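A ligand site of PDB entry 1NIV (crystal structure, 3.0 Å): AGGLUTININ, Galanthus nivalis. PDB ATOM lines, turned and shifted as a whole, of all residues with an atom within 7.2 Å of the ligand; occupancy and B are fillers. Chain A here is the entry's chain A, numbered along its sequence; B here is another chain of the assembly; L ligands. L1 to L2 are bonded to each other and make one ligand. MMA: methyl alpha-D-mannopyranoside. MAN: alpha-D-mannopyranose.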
ATOM      1  N   ILE A  24      -4.801  31.283  -9.604  1.00  0.00           N
ATOM      2  CA  ILE A  24      -4.230  32.405 -10.349  1.00  0.00           C
ATOM      3  C   ILE A  24      -4.111  32.291 -11.864  1.00  0.00           C
ATOM      4  O   ILE A  24      -3.739  31.249 -12.387  1.00  0.00           O
ATOM      5  CB  ILE A  24      -2.846  32.807  -9.772  1.00  0.00           C
ATOM      6  CG1 ILE A  24      -2.278  34.013 -10.515  1.00  0.00           C
ATOM      7  CG2 ILE A  24      -1.901  31.619  -9.798  1.00  0.00           C
ATOM      8  CD1 ILE A  24      -1.042  34.588  -9.877  1.00  0.00           C
ATOM      9  N   GLN A  26      -2.024  33.261 -14.552  1.00  0.00           N
ATOM     10  CA  GLN A  26      -0.654  33.740 -14.750  1.00  0.00           C
ATOM     11  C   GLN A  26      -0.339  34.474 -16.063  1.00  0.00           C
ATOM     12  O   GLN A  26      -1.099  34.419 -17.029  1.00  0.00           O
ATOM     13  CB  GLN A  26       0.315  32.590 -14.535  1.00  0.00           C
ATOM     14  CG  GLN A  26      -0.002  31.760 -13.314  1.00  0.00           C
ATOM     15  CD  GLN A  26       1.033  30.701 -13.023  1.00  0.00           C
ATOM     16  OE1 GLN A  26       1.273  30.366 -11.879  1.00  0.00           O
ATOM     17  NE2 GLN A  26       1.664  30.178 -14.067  1.00  0.00           N
ATOM     18  N   GLU A  27       0.817  35.138 -16.075  1.00  0.00           N
ATOM     19  CA  GLU A  27       1.309  35.880 -17.230  1.00  0.00           C
ATOM     20  C   GLU A  27       1.493  34.976 -18.446  1.00  0.00           C
ATOM     21  O   GLU A  27       1.083  35.307 -19.548  1.00  0.00           O
ATOM     22  CB  GLU A  27       2.624  36.573 -16.856  1.00  0.00           C
ATOM     23  CG  GLU A  27       3.263  37.385 -17.975  1.00  0.00           C
ATOM     24  CD  GLU A  27       2.454  38.596 -18.409  1.00  0.00           C
ATOM     25  OE1 GLU A  27       1.396  38.415 -19.037  1.00  0.00           O
ATOM     26  OE2 GLU A  27       2.892  39.733 -18.131  1.00  0.00           O
ATOM     27  N   ASP A  28       2.063  33.801 -18.215  1.00  0.00           N
ATOM     28  CA  ASP A  28       2.295  32.852 -19.291  1.00  0.00           C
ATOM     29  C   ASP A  28       1.036  32.154 -19.819  1.00  0.00           C
ATOM     30  O   ASP A  28       1.117  31.248 -20.652  1.00  0.00           O
ATOM     31  CB  ASP A  28       3.323  31.806 -18.861  1.00  0.00           C
ATOM     32  CG  ASP A  28       2.847  30.955 -17.703  1.00  0.00           C
ATOM     33  OD1 ASP A  28       1.749  31.191 -17.160  1.00  0.00           O
ATOM     34  OD2 ASP A  28       3.601  30.018 -17.332  1.00  0.00           O
ATOM     35  N   CYS A  29      -0.127  32.580 -19.316  1.00  0.00           N
ATOM     36  CA  CYS A  29      -1.398  32.006 -19.735  1.00  0.00           C
ATOM     37  C   CYS A  29      -1.715  30.676 -19.102  1.00  0.00           C
ATOM     38  O   CYS A  29      -2.515  29.924 -19.636  1.00  0.00           O
ATOM     39  CB  CYS A  29      -1.454  31.866 -21.242  1.00  0.00           C
ATOM     40  SG  CYS A  29      -1.519  33.483 -22.019  1.00  0.00           S
ATOM     41  N   ASN A  30      -1.094  30.381 -17.974  1.00  0.00           N
ATOM     42  CA  ASN A  30      -1.366  29.115 -17.324  1.00  0.00           C
ATOM     43  C   ASN A  30      -2.267  29.388 -16.139  1.00  0.00           C
ATOM     44  O   ASN A  30      -1.912  30.167 -15.255  1.00  0.00           O
ATOM     45  CB  ASN A  30      -0.078  28.445 -16.901  1.00  0.00           C
ATOM     46  CG  ASN A  30      -0.234  26.963 -16.778  1.00  0.00           C
ATOM     47  OD1 ASN A  30      -1.261  26.413 -17.171  1.00  0.00           O
ATOM     48  ND2 ASN A  30       0.791  26.301 -16.263  1.00  0.00           N
ATOM     49  N   LEU A  31      -3.476  28.857 -16.179  1.00  0.00           N
ATOM     50  CA  LEU A  31      -4.407  29.041 -15.075  1.00  0.00           C
ATOM     51  C   LEU A  31      -4.041  27.902 -14.147  1.00  0.00           C
ATOM     52  O   LEU A  31      -4.219  26.740 -14.502  1.00  0.00           O
ATOM     53  CB  LEU A  31      -5.860  28.904 -15.542  1.00  0.00           C
ATOM     54  CG  LEU A  31      -6.990  29.110 -14.527  1.00  0.00           C
ATOM     55  CD1 LEU A  31      -6.866  30.444 -13.813  1.00  0.00           C
ATOM     56  CD2 LEU A  31      -8.335  29.028 -15.230  1.00  0.00           C
ATOM     57  N   VAL A  32      -3.495  28.249 -12.990  1.00  0.00           N
ATOM     58  CA  VAL A  32      -3.052  27.279 -12.000  1.00  0.00           C
ATOM     59  C   VAL A  32      -3.688  27.462 -10.626  1.00  0.00           C
ATOM     60  O   VAL A  32      -4.033  28.572 -10.245  1.00  0.00           O
ATOM     61  CB  VAL A  32      -1.515  27.368 -11.826  1.00  0.00           C
ATOM     62  CG1 VAL A  32      -1.002  26.285 -10.893  1.00  0.00           C
ATOM     63  CG2 VAL A  32      -0.827  27.316 -13.193  1.00  0.00           C
ATOM     64  N   TYR A  34      -2.882  26.803  -6.782  1.00  0.00           N
ATOM     65  CA  TYR A  34      -1.784  26.478  -5.870  1.00  0.00           C
ATOM     66  C   TYR A  34      -2.263  26.313  -4.449  1.00  0.00           C
ATOM     67  O   TYR A  34      -3.210  26.993  -4.026  1.00  0.00           O
ATOM     68  CB  TYR A  34      -0.756  27.619  -5.847  1.00  0.00           C
ATOM     69  CG  TYR A  34       0.041  27.811  -7.103  1.00  0.00           C
ATOM     70  CD1 TYR A  34       1.196  27.062  -7.347  1.00  0.00           C
ATOM     71  CD2 TYR A  34      -0.352  28.765  -8.053  1.00  0.00           C
ATOM     72  CE1 TYR A  34       1.963  27.260  -8.500  1.00  0.00           C
ATOM     73  CE2 TYR A  34       0.391  28.969  -9.209  1.00  0.00           C
ATOM     74  CZ  TYR A  34       1.557  28.213  -9.424  1.00  0.00           C
ATOM     75  OH  TYR A  34       2.285  28.390 -10.581  1.00  0.00           O
ATOM     76  N   ASP A  37       2.742  26.859  -2.049  1.00  0.00           N
ATOM     77  CA  ASP A  37       3.691  26.863  -3.152  1.00  0.00           C
ATOM     78  C   ASP A  37       3.557  25.622  -4.033  1.00  0.00           C
ATOM     79  O   ASP A  37       4.201  25.517  -5.069  1.00  0.00           O
ATOM     80  CB  ASP A  37       5.136  27.019  -2.649  1.00  0.00           C
ATOM     81  CG  ASP A  37       5.599  25.843  -1.785  1.00  0.00           C
ATOM     82  OD1 ASP A  37       4.770  25.192  -1.123  1.00  0.00           O
ATOM     83  OD2 ASP A  37       6.826  25.566  -1.753  1.00  0.00           O
ATOM     84  N   LYS A  38       2.667  24.714  -3.664  1.00  0.00           N
ATOM     85  CA  LYS A  38       2.488  23.489  -4.433  1.00  0.00           C
ATOM     86  C   LYS A  38       1.423  23.639  -5.501  1.00  0.00           C
ATOM     87  O   LYS A  38       0.314  24.079  -5.223  1.00  0.00           O
ATOM     88  CB  LYS A  38       2.086  22.343  -3.511  1.00  0.00           C
ATOM     89  CG  LYS A  38       3.017  22.176  -2.344  1.00  0.00           C
ATOM     90  CD  LYS A  38       2.423  21.257  -1.309  1.00  0.00           C
ATOM     91  CE  LYS A  38       3.303  21.184  -0.077  1.00  0.00           C
ATOM     92  NZ  LYS A  38       2.791  20.209   0.933  1.00  0.00           N
ATOM     93  N   PRO A  39       1.773  23.307  -6.754  1.00  0.00           N
ATOM     94  CA  PRO A  39       0.798  23.405  -7.835  1.00  0.00           C
ATOM     95  C   PRO A  39      -0.179  22.243  -7.622  1.00  0.00           C
ATOM     96  O   PRO A  39       0.261  21.135  -7.278  1.00  0.00           O
ATOM     97  CB  PRO A  39       1.639  23.151  -9.080  1.00  0.00           C
ATOM     98  CG  PRO A  39       3.030  23.510  -8.635  1.00  0.00           C
ATOM     99  CD  PRO A  39       3.084  22.923  -7.285  1.00  0.00           C
ATOM    100  N   ILE A  40      -1.468  22.491  -7.787  1.00  0.00           N
ATOM    101  CA  ILE A  40      -2.481  21.464  -7.570  1.00  0.00           C
ATOM    102  C   ILE A  40      -3.202  21.141  -8.867  1.00  0.00           C
ATOM    103  O   ILE A  40      -3.434  19.982  -9.162  1.00  0.00           O
ATOM    104  CB  ILE A  40      -3.527  21.947  -6.573  1.00  0.00           C
ATOM    105  CG1 ILE A  40      -2.872  22.311  -5.251  1.00  0.00           C
ATOM    106  CG2 ILE A  40      -4.561  20.857  -6.330  1.00  0.00           C
ATOM    107  CD1 ILE A  40      -2.372  21.123  -4.519  1.00  0.00           C
ATOM    108  N   TRP A  41      -3.554  22.169  -9.627  1.00  0.00           N
ATOM    109  CA  TRP A  41      -4.265  21.986 -10.890  1.00  0.00           C
ATOM    110  C   TRP A  41      -3.768  23.044 -11.848  1.00  0.00           C
ATOM    111  O   TRP A  41      -3.207  24.063 -11.429  1.00  0.00           O
ATOM    112  CB  TRP A  41      -5.771  22.160 -10.669  1.00  0.00           C
ATOM    113  CG  TRP A  41      -6.640  21.831 -11.834  1.00  0.00           C
ATOM    114  CD1 TRP A  41      -7.119  20.593 -12.175  1.00  0.00           C
ATOM    115  CD2 TRP A  41      -7.163  22.738 -12.810  1.00  0.00           C
ATOM    116  NE1 TRP A  41      -7.895  20.689 -13.308  1.00  0.00           N
ATOM    117  CE2 TRP A  41      -7.938  21.991 -13.710  1.00  0.00           C
ATOM    118  CE3 TRP A  41      -7.040  24.114 -13.000  1.00  0.00           C
ATOM    119  CZ2 TRP A  41      -8.596  22.571 -14.805  1.00  0.00           C
ATOM    120  CZ3 TRP A  41      -7.690  24.696 -14.083  1.00  0.00           C
ATOM    121  CH2 TRP A  41      -8.465  23.914 -14.969  1.00  0.00           C
ATOM    122  N   ALA A  42      -3.996  22.828 -13.143  1.00  0.00           N
ATOM    123  CA  ALA A  42      -3.536  23.780 -14.132  1.00  0.00           C
ATOM    124  C   ALA A  42      -4.118  23.437 -15.480  1.00  0.00           C
ATOM    125  O   ALA A  42      -4.329  22.276 -15.781  1.00  0.00           O
ATOM    126  CB  ALA A  42      -2.026  23.741 -14.204  1.00  0.00           C
ATOM    127  N   ASN A  44      -2.571  23.810 -18.071  1.00  0.00           N
ATOM    128  CA  ASN A  44      -1.400  23.393 -18.830  1.00  0.00           C
ATOM    129  C   ASN A  44      -1.288  24.087 -20.173  1.00  0.00           C
ATOM    130  O   ASN A  44      -0.884  23.489 -21.158  1.00  0.00           O
ATOM    131  CB  ASN A  44      -1.402  21.879 -18.980  1.00  0.00           C
ATOM    132  CG  ASN A  44      -1.104  21.188 -17.680  1.00  0.00           C
ATOM    133  OD1 ASN A  44      -0.409  21.756 -16.811  1.00  0.00           O
ATOM    134  ND2 ASN A  44      -1.634  19.990 -17.493  1.00  0.00           N
ATOM    135  N   THR A  45      -1.625  25.363 -20.191  1.00  0.00           N
ATOM    136  CA  THR A  45      -1.570  26.166 -21.400  1.00  0.00           C
ATOM    137  C   THR A  45      -0.477  27.203 -21.286  1.00  0.00           C
ATOM    138  O   THR A  45      -0.428  28.140 -22.074  1.00  0.00           O
ATOM    139  CB  THR A  45      -2.900  26.864 -21.622  1.00  0.00           C
ATOM    140  OG1 THR A  45      -3.226  27.633 -20.457  1.00  0.00           O
ATOM    141  CG2 THR A  45      -4.004  25.849 -21.827  1.00  0.00           C
ATOM    142  N   GLY A  46       0.389  27.041 -20.292  1.00  0.00           N
ATOM    143  CA  GLY A  46       1.474  27.976 -20.084  1.00  0.00           C
ATOM    144  C   GLY A  46       2.378  28.058 -21.284  1.00  0.00           C
ATOM    145  O   GLY A  46       2.700  27.046 -21.909  1.00  0.00           O
ATOM    146  N   GLY A  47       2.746  29.281 -21.637  1.00  0.00           N
ATOM    147  CA  GLY A  47       3.610  29.501 -22.772  1.00  0.00           C
ATOM    148  C   GLY A  47       2.860  29.662 -24.071  1.00  0.00           C
ATOM    149  O   GLY A  47       3.410  30.200 -25.016  1.00  0.00           O
ATOM    150  N   ARG A  50       0.763  35.204 -23.807  1.00  0.00           N
ATOM    151  CA  ARG A  50       1.218  36.110 -22.775  1.00  0.00           C
ATOM    152  C   ARG A  50       0.043  37.027 -22.509  1.00  0.00           C
ATOM    153  O   ARG A  50      -0.758  37.257 -23.405  1.00  0.00           O
ATOM    154  CB  ARG A  50       2.418  36.917 -23.264  1.00  0.00           C
ATOM    155  CG  ARG A  50       3.021  37.815 -22.206  1.00  0.00           C
ATOM    156  CD  ARG A  50       4.532  37.855 -22.338  1.00  0.00           C
ATOM    157  NE  ARG A  50       5.106  36.518 -22.427  1.00  0.00           N
ATOM    158  CZ  ARG A  50       5.022  35.591 -21.473  1.00  0.00           C
ATOM    159  NH1 ARG A  50       4.411  35.853 -20.328  1.00  0.00           N
ATOM    160  NH2 ARG A  50       5.531  34.385 -21.683  1.00  0.00           N
ATOM    161  N   VAL B  36       2.420  33.841  -3.299  1.00  0.00           N
ATOM    162  CA  VAL B  36       1.926  32.795  -4.183  1.00  0.00           C
ATOM    163  C   VAL B  36       2.942  31.675  -4.030  1.00  0.00           C
ATOM    164  O   VAL B  36       3.128  31.171  -2.927  1.00  0.00           O
ATOM    165  CB  VAL B  36       1.812  33.213  -5.656  1.00  0.00           C
ATOM    166  CG1 VAL B  36       1.006  32.179  -6.402  1.00  0.00           C
ATOM    167  CG2 VAL B  36       1.134  34.555  -5.792  1.00  0.00           C
ATOM    168  N   ASP B  37       3.686  31.365  -5.089  1.00  0.00           N
ATOM    169  CA  ASP B  37       4.653  30.283  -4.998  1.00  0.00           C
ATOM    170  C   ASP B  37       6.081  30.789  -4.804  1.00  0.00           C
ATOM    171  O   ASP B  37       7.001  30.007  -4.598  1.00  0.00           O
ATOM    172  CB  ASP B  37       4.560  29.349  -6.225  1.00  0.00           C
ATOM    173  CG  ASP B  37       4.934  30.049  -7.534  1.00  0.00           C
ATOM    174  OD1 ASP B  37       4.752  31.274  -7.659  1.00  0.00           O
ATOM    175  OD2 ASP B  37       5.412  29.358  -8.471  1.00  0.00           O
ATOM    176  N   LYS B  38       6.261  32.101  -4.796  1.00  0.00           N
ATOM    177  CA  LYS B  38       7.587  32.664  -4.642  1.00  0.00           C
ATOM    178  C   LYS B  38       7.931  32.934  -3.185  1.00  0.00           C
ATOM    179  O   LYS B  38       7.156  33.553  -2.468  1.00  0.00           O
ATOM    180  CB  LYS B  38       7.688  33.980  -5.405  1.00  0.00           C
ATOM    181  CG  LYS B  38       7.263  33.860  -6.840  1.00  0.00           C
ATOM    182  CD  LYS B  38       7.089  35.226  -7.461  1.00  0.00           C
ATOM    183  CE  LYS B  38       6.534  35.108  -8.881  1.00  0.00           C
ATOM    184  NZ  LYS B  38       6.437  36.435  -9.552  1.00  0.00           N
HETATM  185  C1  MMA L   1       4.138  26.178 -15.721  1.00  0.00           C
HETATM  186  C2  MMA L   1       4.138  27.593 -15.182  1.00  0.00           C
HETATM  187  C3  MMA L   1       4.404  27.565 -13.674  1.00  0.00           C
HETATM  188  C4  MMA L   1       3.410  26.642 -12.986  1.00  0.00           C
HETATM  189  C5  MMA L   1       3.408  25.268 -13.643  1.00  0.00           C
HETATM  190  C6  MMA L   1       2.362  24.330 -13.107  1.00  0.00           C
HETATM  191  C7  MMA L   1       5.484  24.216 -15.883  1.00  0.00           C
HETATM  192  O1  MMA L   1       5.370  25.601 -15.503  1.00  0.00           O
HETATM  193  O2  MMA L   1       2.870  28.189 -15.441  1.00  0.00           O
HETATM  194  O3  MMA L   1       4.272  28.885 -13.140  1.00  0.00           O
HETATM  195  O4  MMA L   1       3.786  26.522 -11.624  1.00  0.00           O
HETATM  196  O5  MMA L   1       3.152  25.388 -15.040  1.00  0.00           O
HETATM  197  O6  MMA L   1       2.309  23.149 -13.898  1.00  0.00           O
HETATM  198  C1  MAN L   2       5.217  29.265 -12.172  1.00  0.00           C
HETATM  199  C2  MAN L   2       5.037  30.739 -11.845  1.00  0.00           C
HETATM  200  C3  MAN L   2       5.278  31.531 -13.121  1.00  0.00           C
HETATM  201  C4  MAN L   2       6.658  31.225 -13.678  1.00  0.00           C
HETATM  202  C5  MAN L   2       6.837  29.737 -13.848  1.00  0.00           C
HETATM  203  C6  MAN L   2       8.260  29.351 -14.238  1.00  0.00           C
HETATM  204  O2  MAN L   2       5.966  31.141 -10.837  1.00  0.00           O
HETATM  205  O3  MAN L   2       5.155  32.918 -12.856  1.00  0.00           O
HETATM  206  O4  MAN L   2       6.804  31.848 -14.952  1.00  0.00           O
HETATM  207  O5  MAN L   2       6.538  29.066 -12.620  1.00  0.00           O
HETATM  208  O6  MAN L   2       8.358  27.946 -14.508  1.00  0.00           O
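Hydrophobic or aromatic side chains within 4 Å of the ligand: Tyr 34. Within 4 Å of the ligand: Gln 26, Asp 28, Asn 30, Tyr 34 and Asp 37 of chain B.
The side-chain carboxylate of Asp 28 sits at hydrogen-bond distance from the backbone NH of Asn 30, at 3.1 Å. O of Asp 28 sits at hydrogen-bond distance from N of Gly 47 (2.7 Å). OH of Tyr 34 lies within hydrogen-bond range of OE1 of Gln 26, at 2.6 Å. The backbone NH of Thr 45 sits at hydrogen-bond distance from the side-chain amide oxygen of Asn 30, at 3.2 Å. The side-chain amide nitrogen (NE2) of Gln 26 is in hydrogen-bond range of the side-chain carboxylate (OD1) of Asp 28 (3.3 Å). N of Asn 44 sits at hydrogen-bond distance from OD1 of Asn 30, at 3.0 Å.
An oxygen (O5) of MMA L1 is in hydrogen-bond range of the side-chain amide nitrogen of Asn 30 (2.8 Å). O4 of MMA L1 sits at hydrogen-bond distance from OH of Tyr 34, at 2.6 Å. The side-chain carboxylate (OD2) of Asp 28 is in hydrogen-bond range of an oxygen (O2) of MMA L1 (2.7 Å). An oxygen (O2) of MAN L2 is in hydrogen-bond range of the side-chain carboxylate of Asp 37 of chain B (3.0 Å). O2 of MMA L1 sits at hydrogen-bond distance from NE2 of Gln 26.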
